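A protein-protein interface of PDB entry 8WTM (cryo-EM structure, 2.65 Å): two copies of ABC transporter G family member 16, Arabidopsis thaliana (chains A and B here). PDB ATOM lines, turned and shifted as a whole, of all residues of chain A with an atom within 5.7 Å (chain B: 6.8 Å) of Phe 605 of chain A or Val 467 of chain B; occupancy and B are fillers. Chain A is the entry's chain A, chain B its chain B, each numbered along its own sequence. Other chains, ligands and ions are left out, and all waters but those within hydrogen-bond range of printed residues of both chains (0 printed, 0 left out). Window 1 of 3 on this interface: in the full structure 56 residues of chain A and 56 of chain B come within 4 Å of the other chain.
CG2 of Ile 463 of chain B touches CE1 of Tyr 601 of chain A, 3.9 Å away. Leu 604 of chain A touches Leu 464 of chain B. Phe 468 of chain B touches Leu 604 of chain A (CE2 to CD1, 3.9 Å). Phe 605 of chain A touches Val 467 of chain B (CZ to CG2, 3.5 Å). Ile 610 of chain A touches Val 467 of chain B (CD1 to O, 3.8 Å). Ile 610 of chain A touches Glu 480 of chain B (CG1 to OE2, 3.8 Å). Pro 616 of chain A touches Thr 466 of chain B (CG to O, 3.5 Å). CD of Pro 616 of chain A touches O of Val 467 of chain B, at 3.6 Å. Tyr 618 of chain A touches Trp 469 of chain B. Trp 619 of chain A touches Val 467 of chain B (CD1 to CG2, 3.6 Å).
Of chain A, only Phe 605 (3.5 Å), Ile 610 (3.8 Å), Pro 616 (3.6 Å) and Trp 619 (3.6 Å) come within 4 Å of Val 467 of chain B. Printed residues of chain B within 4 Å of Ile 610 of chain A: Val 467 (3.8 Å) and Glu 480 (3.8 Å). Of the printed residues of chain A, Phe 468 of chain B touches Leu 604. Printed residues of chain B within 4 Å of Trp 619 of chain A: Thr 466 (2.9 Å) and Val 467 (3.6 Å). Printed residues of chain B within 4 Å of Tyr 618 of chain A: Thr 466 (3.0 Å) and Trp 469 (3.98 Å). Phe 608 of chain A touches none of the printed residues of chain B. Ser 606 of chain A touches none of the printed residues of chain B. The nearest residue of chain B that does not touch Phe 605 of chain A is Ile 463 of chain B (4.6 Å).
The guanidinium group (NE) of Arg 614 of chain A is in salt-bridge range of the side-chain carboxylate (OE2) of Glu 480 of chain B (3.4 Å). O of Thr 466 of chain B lies within hydrogen-bond range of OH of Tyr 618 of chain A (3.0 Å). NE1 of Trp 619 of chain A is in hydrogen-bond range of OG1 of Thr 466 of chain B (2.9 Å).
No position is printed for both chains.
Printed residues of chain B that touch a printed residue of chain A: Ile 463, Leu 464, Thr 466, Val 467, Phe 468, Trp 469 and Glu 480. Along chain B the printed residues that touch a printed residue of chain A span positions 463 to 480.
The backbone carbonyl oxygen (O) of Phe 605 of chain A sits at hydrogen-bond distance from a ring nitrogen (ND1) of His 623 of chain A (2.6 Å). OG1 of Thr 466 of chain B lies within hydrogen-bond range of O of Phe 462 of chain B. The backbone carbonyl oxygen of Ile 463 of chain B sits at hydrogen-bond distance from the side-chain hydroxyl of Thr 466 of chain B (3.0 Å).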
ATOM      1  N   ALA A 600      28.289   3.518 -13.228  1.00  0.00           N
ATOM      2  CA  ALA A 600      28.867   4.259 -14.342  1.00  0.00           C
ATOM      3  C   ALA A 600      27.900   5.282 -14.915  1.00  0.00           C
ATOM      4  O   ALA A 600      28.319   6.382 -15.280  1.00  0.00           O
ATOM      5  CB  ALA A 600      29.304   3.290 -15.430  1.00  0.00           C
ATOM      6  N   TYR A 601      26.617   4.951 -14.989  1.00  0.00           N
ATOM      7  CA  TYR A 601      25.617   5.904 -15.443  1.00  0.00           C
ATOM      8  C   TYR A 601      25.175   6.857 -14.349  1.00  0.00           C
ATOM      9  O   TYR A 601      24.640   7.918 -14.657  1.00  0.00           O
ATOM     10  CB  TYR A 601      24.417   5.165 -16.020  1.00  0.00           C
ATOM     11  CG  TYR A 601      24.739   4.540 -17.343  1.00  0.00           C
ATOM     12  CD1 TYR A 601      25.097   5.325 -18.426  1.00  0.00           C
ATOM     13  CD2 TYR A 601      24.719   3.169 -17.506  1.00  0.00           C
ATOM     14  CE1 TYR A 601      25.413   4.762 -19.632  1.00  0.00           C
ATOM     15  CE2 TYR A 601      25.033   2.598 -18.711  1.00  0.00           C
ATOM     16  CZ  TYR A 601      25.380   3.400 -19.768  1.00  0.00           C
ATOM     17  OH  TYR A 601      25.689   2.837 -20.973  1.00  0.00           O
ATOM     18  N   PHE A 602      25.390   6.513 -13.082  1.00  0.00           N
ATOM     19  CA  PHE A 602      25.196   7.487 -12.020  1.00  0.00           C
ATOM     20  C   PHE A 602      26.256   8.573 -12.076  1.00  0.00           C
ATOM     21  O   PHE A 602      26.000   9.708 -11.668  1.00  0.00           O
ATOM     22  CB  PHE A 602      25.227   6.799 -10.658  1.00  0.00           C
ATOM     23  CG  PHE A 602      23.956   6.101 -10.290  1.00  0.00           C
ATOM     24  CD1 PHE A 602      22.777   6.373 -10.957  1.00  0.00           C
ATOM     25  CD2 PHE A 602      23.944   5.164  -9.274  1.00  0.00           C
ATOM     26  CE1 PHE A 602      21.618   5.736 -10.617  1.00  0.00           C
ATOM     27  CE2 PHE A 602      22.786   4.516  -8.938  1.00  0.00           C
ATOM     28  CZ  PHE A 602      21.620   4.813  -9.605  1.00  0.00           C
ATOM     29  N   LEU A 603      27.445   8.240 -12.570  1.00  0.00           N
ATOM     30  CA  LEU A 603      28.528   9.199 -12.708  1.00  0.00           C
ATOM     31  C   LEU A 603      28.392  10.043 -13.969  1.00  0.00           C
ATOM     32  O   LEU A 603      28.768  11.219 -13.963  1.00  0.00           O
ATOM     33  CB  LEU A 603      29.858   8.453 -12.692  1.00  0.00           C
ATOM     34  CG  LEU A 603      31.151   9.260 -12.744  1.00  0.00           C
ATOM     35  CD1 LEU A 603      31.241  10.242 -11.599  1.00  0.00           C
ATOM     36  CD2 LEU A 603      32.343   8.340 -12.768  1.00  0.00           C
ATOM     37  N   LEU A 604      27.853   9.472 -15.047  1.00  0.00           N
ATOM     38  CA  LEU A 604      27.593  10.244 -16.255  1.00  0.00           C
ATOM     39  C   LEU A 604      26.505  11.287 -16.033  1.00  0.00           C
ATOM     40  O   LEU A 604      26.541  12.358 -16.645  1.00  0.00           O
ATOM     41  CB  LEU A 604      27.213   9.302 -17.397  1.00  0.00           C
ATOM     42  CG  LEU A 604      27.033   9.895 -18.796  1.00  0.00           C
ATOM     43  CD1 LEU A 604      28.362  10.275 -19.391  1.00  0.00           C
ATOM     44  CD2 LEU A 604      26.314   8.932 -19.690  1.00  0.00           C
ATOM     45  N   PHE A 605      25.556  11.011 -15.142  1.00  0.00           N
ATOM     46  CA  PHE A 605      24.440  11.901 -14.871  1.00  0.00           C
ATOM     47  C   PHE A 605      24.577  12.644 -13.550  1.00  0.00           C
ATOM     48  O   PHE A 605      23.601  13.219 -13.076  1.00  0.00           O
ATOM     49  CB  PHE A 605      23.133  11.116 -14.892  1.00  0.00           C
ATOM     50  CG  PHE A 605      22.681  10.735 -16.268  1.00  0.00           C
ATOM     51  CD1 PHE A 605      21.860  11.574 -16.993  1.00  0.00           C
ATOM     52  CD2 PHE A 605      23.078   9.541 -16.838  1.00  0.00           C
ATOM     53  CE1 PHE A 605      21.443  11.226 -18.250  1.00  0.00           C
ATOM     54  CE2 PHE A 605      22.664   9.190 -18.090  1.00  0.00           C
ATOM     55  CZ  PHE A 605      21.845  10.031 -18.794  1.00  0.00           C
ATOM     56  N   SER A 606      25.766  12.659 -12.956  1.00  0.00           N
ATOM     57  CA  SER A 606      25.982  13.333 -11.685  1.00  0.00           C
ATOM     58  C   SER A 606      26.210  14.830 -11.821  1.00  0.00           C
ATOM     59  O   SER A 606      26.275  15.519 -10.802  1.00  0.00           O
ATOM     60  CB  SER A 606      27.175  12.719 -10.963  1.00  0.00           C
ATOM     61  OG  SER A 606      28.361  12.919 -11.699  1.00  0.00           O
ATOM     62  N   GLY A 607      26.326  15.353 -13.035  1.00  0.00           N
ATOM     63  CA  GLY A 607      26.672  16.738 -13.241  1.00  0.00           C
ATOM     64  C   GLY A 607      28.142  17.004 -13.464  1.00  0.00           C
ATOM     65  O   GLY A 607      28.517  18.159 -13.665  1.00  0.00           O
ATOM     66  N   PHE A 608      28.983  15.976 -13.439  1.00  0.00           N
ATOM     67  CA  PHE A 608      30.411  16.153 -13.661  1.00  0.00           C
ATOM     68  C   PHE A 608      30.788  16.069 -15.135  1.00  0.00           C
ATOM     69  O   PHE A 608      31.563  16.897 -15.617  1.00  0.00           O
ATOM     70  CB  PHE A 608      31.205  15.116 -12.864  1.00  0.00           C
ATOM     71  CG  PHE A 608      32.663  15.109 -13.184  1.00  0.00           C
ATOM     72  CD1 PHE A 608      33.460  16.178 -12.825  1.00  0.00           C
ATOM     73  CD2 PHE A 608      33.237  14.047 -13.860  1.00  0.00           C
ATOM     74  CE1 PHE A 608      34.797  16.188 -13.131  1.00  0.00           C
ATOM     75  CE2 PHE A 608      34.573  14.054 -14.169  1.00  0.00           C
ATOM     76  CZ  PHE A 608      35.355  15.124 -13.799  1.00  0.00           C
ATOM     77  N   ILE A 610      28.570  16.216 -17.759  1.00  0.00           N
ATOM     78  CA  ILE A 610      27.749  17.229 -18.405  1.00  0.00           C
ATOM     79  C   ILE A 610      26.886  17.861 -17.324  1.00  0.00           C
ATOM     80  O   ILE A 610      26.298  17.154 -16.503  1.00  0.00           O
ATOM     81  CB  ILE A 610      26.923  16.627 -19.568  1.00  0.00           C
ATOM     82  CG1 ILE A 610      25.929  17.633 -20.140  1.00  0.00           C
ATOM     83  CG2 ILE A 610      26.245  15.318 -19.174  1.00  0.00           C
ATOM     84  CD1 ILE A 610      25.284  17.168 -21.399  1.00  0.00           C
ATOM     85  N   ARG A 614      22.738  21.671 -18.845  1.00  0.00           N
ATOM     86  CA  ARG A 614      23.046  21.276 -20.210  1.00  0.00           C
ATOM     87  C   ARG A 614      22.506  19.907 -20.583  1.00  0.00           C
ATOM     88  O   ARG A 614      22.493  19.578 -21.770  1.00  0.00           O
ATOM     89  CB  ARG A 614      24.560  21.291 -20.437  1.00  0.00           C
ATOM     90  CG  ARG A 614      25.208  22.625 -20.181  1.00  0.00           C
ATOM     91  CD  ARG A 614      24.990  23.569 -21.336  1.00  0.00           C
ATOM     92  NE  ARG A 614      25.711  23.138 -22.523  1.00  0.00           N
ATOM     93  CZ  ARG A 614      26.010  23.931 -23.542  1.00  0.00           C
ATOM     94  NH1 ARG A 614      25.654  25.203 -23.517  1.00  0.00           N
ATOM     95  NH2 ARG A 614      26.669  23.452 -24.584  1.00  0.00           N
ATOM     96  N   ILE A 615      22.073  19.110 -19.614  1.00  0.00           N
ATOM     97  CA  ILE A 615      21.472  17.795 -19.876  1.00  0.00           C
ATOM     98  C   ILE A 615      20.139  17.994 -20.588  1.00  0.00           C
ATOM     99  O   ILE A 615      19.389  18.917 -20.225  1.00  0.00           O
ATOM    100  CB  ILE A 615      21.302  17.023 -18.559  1.00  0.00           C
ATOM    101  CG1 ILE A 615      22.659  16.615 -18.006  1.00  0.00           C
ATOM    102  CG2 ILE A 615      20.485  15.765 -18.724  1.00  0.00           C
ATOM    103  CD1 ILE A 615      22.621  16.081 -16.608  1.00  0.00           C
ATOM    104  N   PRO A 616      19.835  17.219 -21.638  1.00  0.00           N
ATOM    105  CA  PRO A 616      18.534  17.343 -22.304  1.00  0.00           C
ATOM    106  C   PRO A 616      17.381  17.000 -21.378  1.00  0.00           C
ATOM    107  O   PRO A 616      17.529  16.234 -20.427  1.00  0.00           O
ATOM    108  CB  PRO A 616      18.633  16.340 -23.452  1.00  0.00           C
ATOM    109  CG  PRO A 616      20.067  16.167 -23.682  1.00  0.00           C
ATOM    110  CD  PRO A 616      20.732  16.310 -22.367  1.00  0.00           C
ATOM    111  N   TYR A 618      14.692  15.289 -21.826  1.00  0.00           N
ATOM    112  CA  TYR A 618      14.227  13.911 -21.825  1.00  0.00           C
ATOM    113  C   TYR A 618      15.145  12.979 -21.045  1.00  0.00           C
ATOM    114  O   TYR A 618      14.852  11.787 -20.949  1.00  0.00           O
ATOM    115  CB  TYR A 618      14.057  13.400 -23.260  1.00  0.00           C
ATOM    116  CG  TYR A 618      15.210  13.684 -24.194  1.00  0.00           C
ATOM    117  CD1 TYR A 618      16.316  12.847 -24.237  1.00  0.00           C
ATOM    118  CD2 TYR A 618      15.180  14.772 -25.053  1.00  0.00           C
ATOM    119  CE1 TYR A 618      17.360  13.092 -25.083  1.00  0.00           C
ATOM    120  CE2 TYR A 618      16.228  15.023 -25.907  1.00  0.00           C
ATOM    121  CZ  TYR A 618      17.313  14.175 -25.918  1.00  0.00           C
ATOM    122  OH  TYR A 618      18.363  14.410 -26.762  1.00  0.00           O
ATOM    123  N   TRP A 619      16.237  13.489 -20.487  1.00  0.00           N
ATOM    124  CA  TRP A 619      17.127  12.707 -19.648  1.00  0.00           C
ATOM    125  C   TRP A 619      17.242  13.247 -18.235  1.00  0.00           C
ATOM    126  O   TRP A 619      17.952  12.650 -17.422  1.00  0.00           O
ATOM    127  CB  TRP A 619      18.530  12.643 -20.261  1.00  0.00           C
ATOM    128  CG  TRP A 619      18.752  11.531 -21.229  1.00  0.00           C
ATOM    129  CD1 TRP A 619      19.122  11.657 -22.520  1.00  0.00           C
ATOM    130  CD2 TRP A 619      18.646  10.125 -20.977  1.00  0.00           C
ATOM    131  NE1 TRP A 619      19.246  10.430 -23.101  1.00  0.00           N
ATOM    132  CE2 TRP A 619      18.960   9.468 -22.173  1.00  0.00           C
ATOM    133  CE3 TRP A 619      18.320   9.360 -19.853  1.00  0.00           C
ATOM    134  CZ2 TRP A 619      18.951   8.085 -22.286  1.00  0.00           C
ATOM    135  CZ3 TRP A 619      18.312   7.995 -19.968  1.00  0.00           C
ATOM    136  CH2 TRP A 619      18.625   7.368 -21.174  1.00  0.00           C
ATOM    137  N   PHE A 622      16.615  11.076 -14.934  1.00  0.00           N
ATOM    138  CA  PHE A 622      17.653  10.191 -14.440  1.00  0.00           C
ATOM    139  C   PHE A 622      18.785  10.943 -13.764  1.00  0.00           C
ATOM    140  O   PHE A 622      19.555  10.337 -13.016  1.00  0.00           O
ATOM    141  CB  PHE A 622      18.209   9.336 -15.582  1.00  0.00           C
ATOM    142  CG  PHE A 622      18.990   8.154 -15.113  1.00  0.00           C
ATOM    143  CD1 PHE A 622      18.352   7.069 -14.552  1.00  0.00           C
ATOM    144  CD2 PHE A 622      20.366   8.144 -15.190  1.00  0.00           C
ATOM    145  CE1 PHE A 622      19.075   5.992 -14.098  1.00  0.00           C
ATOM    146  CE2 PHE A 622      21.091   7.073 -14.736  1.00  0.00           C
ATOM    147  CZ  PHE A 622      20.448   5.997 -14.195  1.00  0.00           C
ATOM    148  N   HIS A 623      18.902  12.241 -14.020  1.00  0.00           N
ATOM    149  CA  HIS A 623      19.835  13.069 -13.273  1.00  0.00           C
ATOM    150  C   HIS A 623      19.430  13.159 -11.809  1.00  0.00           C
ATOM    151  O   HIS A 623      20.264  12.983 -10.919  1.00  0.00           O
ATOM    152  CB  HIS A 623      19.905  14.453 -13.913  1.00  0.00           C
ATOM    153  CG  HIS A 623      20.721  15.437 -13.140  1.00  0.00           C
ATOM    154  ND1 HIS A 623      22.093  15.369 -13.071  1.00  0.00           N
ATOM    155  CD2 HIS A 623      20.359  16.510 -12.405  1.00  0.00           C
ATOM    156  CE1 HIS A 623      22.542  16.358 -12.323  1.00  0.00           C
ATOM    157  NE2 HIS A 623      21.509  17.061 -11.901  1.00  0.00           N
ATOM    158  N   TYR A 624      18.145  13.378 -11.540  1.00  0.00           N
ATOM    159  CA  TYR A 624      17.662  13.505 -10.174  1.00  0.00           C
ATOM    160  C   TYR A 624      17.555  12.171  -9.454  1.00  0.00           C
ATOM    161  O   TYR A 624      17.424  12.155  -8.229  1.00  0.00           O
ATOM    162  CB  TYR A 624      16.311  14.212 -10.169  1.00  0.00           C
ATOM    163  CG  TYR A 624      16.422  15.684 -10.441  1.00  0.00           C
ATOM    164  CD1 TYR A 624      16.989  16.535  -9.508  1.00  0.00           C
ATOM    165  CD2 TYR A 624      15.973  16.224 -11.632  1.00  0.00           C
ATOM    166  CE1 TYR A 624      17.100  17.877  -9.752  1.00  0.00           C
ATOM    167  CE2 TYR A 624      16.082  17.565 -11.885  1.00  0.00           C
ATOM    168  CZ  TYR A 624      16.644  18.384 -10.943  1.00  0.00           C
ATOM    169  OH  TYR A 624      16.756  19.723 -11.185  1.00  0.00           O
ATOM    170  N   SER A 626      20.085  10.008  -9.707  1.00  0.00           N
ATOM    171  CA  SER A 626      21.467   9.562  -9.635  1.00  0.00           C
ATOM    172  C   SER A 626      21.939   9.545  -8.192  1.00  0.00           C
ATOM    173  O   SER A 626      21.783  10.532  -7.468  1.00  0.00           O
ATOM    174  CB  SER A 626      22.355  10.473 -10.478  1.00  0.00           C
ATOM    175  OG  SER A 626      23.717  10.128 -10.364  1.00  0.00           O
ATOM    176  N   LYS A 629      24.975  12.074  -7.636  1.00  0.00           N
ATOM    177  CA  LYS A 629      24.755  13.513  -7.792  1.00  0.00           C
ATOM    178  C   LYS A 629      24.676  14.242  -6.455  1.00  0.00           C
ATOM    179  O   LYS A 629      25.300  15.292  -6.275  1.00  0.00           O
ATOM    180  CB  LYS A 629      23.476  13.756  -8.595  1.00  0.00           C
ATOM    181  CG  LYS A 629      22.881  15.142  -8.418  1.00  0.00           C
ATOM    182  CD  LYS A 629      21.461  15.207  -8.877  1.00  0.00           C
ATOM    183  CE  LYS A 629      20.738  16.401  -8.307  1.00  0.00           C
ATOM    184  NZ  LYS A 629      21.192  17.699  -8.833  1.00  0.00           N
ATOM    185  N   PHE B 462      23.761   4.549 -27.906  1.00  0.00           N
ATOM    186  CA  PHE B 462      22.520   5.305 -28.033  1.00  0.00           C
ATOM    187  C   PHE B 462      22.307   6.237 -26.849  1.00  0.00           C
ATOM    188  O   PHE B 462      21.761   7.329 -27.017  1.00  0.00           O
ATOM    189  CB  PHE B 462      21.330   4.355 -28.178  1.00  0.00           C
ATOM    190  CG  PHE B 462      19.998   5.047 -28.174  1.00  0.00           C
ATOM    191  CD1 PHE B 462      19.551   5.711 -29.300  1.00  0.00           C
ATOM    192  CD2 PHE B 462      19.192   5.037 -27.042  1.00  0.00           C
ATOM    193  CE1 PHE B 462      18.333   6.354 -29.301  1.00  0.00           C
ATOM    194  CE2 PHE B 462      17.979   5.683 -27.034  1.00  0.00           C
ATOM    195  CZ  PHE B 462      17.547   6.339 -28.166  1.00  0.00           C
ATOM    196  N   ILE B 463      22.701   5.813 -25.650  1.00  0.00           N
ATOM    197  CA  ILE B 463      22.584   6.669 -24.474  1.00  0.00           C
ATOM    198  C   ILE B 463      23.517   7.865 -24.597  1.00  0.00           C
ATOM    199  O   ILE B 463      23.111   9.011 -24.387  1.00  0.00           O
ATOM    200  CB  ILE B 463      22.857   5.857 -23.196  1.00  0.00           C
ATOM    201  CG1 ILE B 463      21.681   4.939 -22.888  1.00  0.00           C
ATOM    202  CG2 ILE B 463      23.133   6.759 -22.014  1.00  0.00           C
ATOM    203  CD1 ILE B 463      21.978   3.916 -21.830  1.00  0.00           C
ATOM    204  N   LEU B 464      24.768   7.619 -24.989  1.00  0.00           N
ATOM    205  CA  LEU B 464      25.757   8.683 -25.118  1.00  0.00           C
ATOM    206  C   LEU B 464      25.427   9.646 -26.245  1.00  0.00           C
ATOM    207  O   LEU B 464      25.779  10.822 -26.170  1.00  0.00           O
ATOM    208  CB  LEU B 464      27.135   8.081 -25.353  1.00  0.00           C
ATOM    209  CG  LEU B 464      27.819   7.412 -24.175  1.00  0.00           C
ATOM    210  CD1 LEU B 464      29.140   6.864 -24.621  1.00  0.00           C
ATOM    211  CD2 LEU B 464      28.009   8.421 -23.088  1.00  0.00           C
ATOM    212  N   ALA B 465      24.771   9.170 -27.293  1.00  0.00           N
ATOM    213  CA  ALA B 465      24.422  10.025 -28.413  1.00  0.00           C
ATOM    214  C   ALA B 465      23.225  10.914 -28.126  1.00  0.00           C
ATOM    215  O   ALA B 465      23.080  11.955 -28.767  1.00  0.00           O
ATOM    216  CB  ALA B 465      24.137   9.177 -29.644  1.00  0.00           C
ATOM    217  N   THR B 466      22.357  10.528 -27.197  1.00  0.00           N
ATOM    218  CA  THR B 466      21.204  11.341 -26.845  1.00  0.00           C
ATOM    219  C   THR B 466      21.480  12.271 -25.673  1.00  0.00           C
ATOM    220  O   THR B 466      20.787  13.277 -25.516  1.00  0.00           O
ATOM    221  CB  THR B 466      20.005  10.446 -26.531  1.00  0.00           C
ATOM    222  OG1 THR B 466      20.387   9.450 -25.580  1.00  0.00           O
ATOM    223  CG2 THR B 466      19.520   9.766 -27.778  1.00  0.00           C
ATOM    224  N   VAL B 467      22.472  11.956 -24.846  1.00  0.00           N
ATOM    225  CA  VAL B 467      22.900  12.875 -23.801  1.00  0.00           C
ATOM    226  C   VAL B 467      23.777  13.966 -24.393  1.00  0.00           C
ATOM    227  O   VAL B 467      23.600  15.155 -24.116  1.00  0.00           O
ATOM    228  CB  VAL B 467      23.629  12.104 -22.687  1.00  0.00           C
ATOM    229  CG1 VAL B 467      24.240  13.048 -21.677  1.00  0.00           C
ATOM    230  CG2 VAL B 467      22.682  11.195 -22.017  1.00  0.00           C
ATOM    231  N   PHE B 468      24.728  13.576 -25.232  1.00  0.00           N
ATOM    232  CA  PHE B 468      25.661  14.497 -25.866  1.00  0.00           C
ATOM    233  C   PHE B 468      25.212  14.852 -27.271  1.00  0.00           C
ATOM    234  O   PHE B 468      26.028  14.983 -28.176  1.00  0.00           O
ATOM    235  CB  PHE B 468      27.061  13.905 -25.878  1.00  0.00           C
ATOM    236  CG  PHE B 468      27.649  13.709 -24.520  1.00  0.00           C
ATOM    237  CD1 PHE B 468      28.134  14.781 -23.799  1.00  0.00           C
ATOM    238  CD2 PHE B 468      27.733  12.447 -23.969  1.00  0.00           C
ATOM    239  CE1 PHE B 468      28.686  14.593 -22.552  1.00  0.00           C
ATOM    240  CE2 PHE B 468      28.282  12.260 -22.731  1.00  0.00           C
ATOM    241  CZ  PHE B 468      28.760  13.334 -22.025  1.00  0.00           C
ATOM    242  N   TRP B 469      23.907  15.000 -27.461  1.00  0.00           N
ATOM    243  CA  TRP B 469      23.306  15.254 -28.762  1.00  0.00           C
ATOM    244  C   TRP B 469      23.676  16.644 -29.259  1.00  0.00           C
ATOM    245  O   TRP B 469      23.252  17.643 -28.674  1.00  0.00           O
ATOM    246  CB  TRP B 469      21.793  15.102 -28.664  1.00  0.00           C
ATOM    247  CG  TRP B 469      21.060  15.440 -29.918  1.00  0.00           C
ATOM    248  CD1 TRP B 469      20.542  16.652 -30.269  1.00  0.00           C
ATOM    249  CD2 TRP B 469      20.754  14.552 -30.987  1.00  0.00           C
ATOM    250  NE1 TRP B 469      19.944  16.573 -31.493  1.00  0.00           N
ATOM    251  CE2 TRP B 469      20.055  15.291 -31.955  1.00  0.00           C
ATOM    252  CE3 TRP B 469      20.999  13.200 -31.220  1.00  0.00           C
ATOM    253  CZ2 TRP B 469      19.604  14.726 -33.136  1.00  0.00           C
ATOM    254  CZ3 TRP B 469      20.550  12.642 -32.390  1.00  0.00           C
ATOM    255  CH2 TRP B 469      19.863  13.401 -33.335  1.00  0.00           C
ATOM    256  N   ARG B 470      24.467  16.690 -30.336  1.00  0.00           N
ATOM    257  CA  ARG B 470      24.720  17.880 -31.155  1.00  0.00           C
ATOM    258  C   ARG B 470      25.322  19.024 -30.343  1.00  0.00           C
ATOM    259  O   ARG B 470      24.719  20.082 -30.175  1.00  0.00           O
ATOM    260  CB  ARG B 470      23.444  18.325 -31.870  1.00  0.00           C
ATOM    261  CG  ARG B 470      23.091  17.465 -33.048  1.00  0.00           C
ATOM    262  CD  ARG B 470      24.107  17.659 -34.121  1.00  0.00           C
ATOM    263  NE  ARG B 470      24.002  16.674 -35.184  1.00  0.00           N
ATOM    264  CZ  ARG B 470      24.679  16.751 -36.321  1.00  0.00           C
ATOM    265  NH1 ARG B 470      25.501  17.770 -36.536  1.00  0.00           N
ATOM    266  NH2 ARG B 470      24.539  15.814 -37.244  1.00  0.00           N
ATOM    267  N   LEU B 471      26.525  18.782 -29.834  1.00  0.00           N
ATOM    268  CA  LEU B 471      27.194  19.737 -28.963  1.00  0.00           C
ATOM    269  C   LEU B 471      27.597  20.993 -29.725  1.00  0.00           C
ATOM    270  O   LEU B 471      28.047  20.928 -30.869  1.00  0.00           O
ATOM    271  CB  LEU B 471      28.424  19.091 -28.331  1.00  0.00           C
ATOM    272  CG  LEU B 471      28.186  17.773 -27.607  1.00  0.00           C
ATOM    273  CD1 LEU B 471      29.496  17.113 -27.268  1.00  0.00           C
ATOM    274  CD2 LEU B 471      27.377  18.011 -26.362  1.00  0.00           C
ATOM    275  N   GLU B 480      32.277  19.269 -22.588  1.00  0.00           N
ATOM    276  CA  GLU B 480      31.412  18.122 -22.814  1.00  0.00           C
ATOM    277  C   GLU B 480      31.936  17.203 -23.902  1.00  0.00           C
ATOM    278  O   GLU B 480      31.577  16.026 -23.921  1.00  0.00           O
ATOM    279  CB  GLU B 480      30.002  18.583 -23.171  1.00  0.00           C
ATOM    280  CG  GLU B 480      29.147  18.885 -21.977  1.00  0.00           C
ATOM    281  CD  GLU B 480      28.150  19.991 -22.233  1.00  0.00           C
ATOM    282  OE1 GLU B 480      27.712  20.146 -23.386  1.00  0.00           O
ATOM    283  OE2 GLU B 480      27.814  20.717 -21.277  1.00  0.00           O
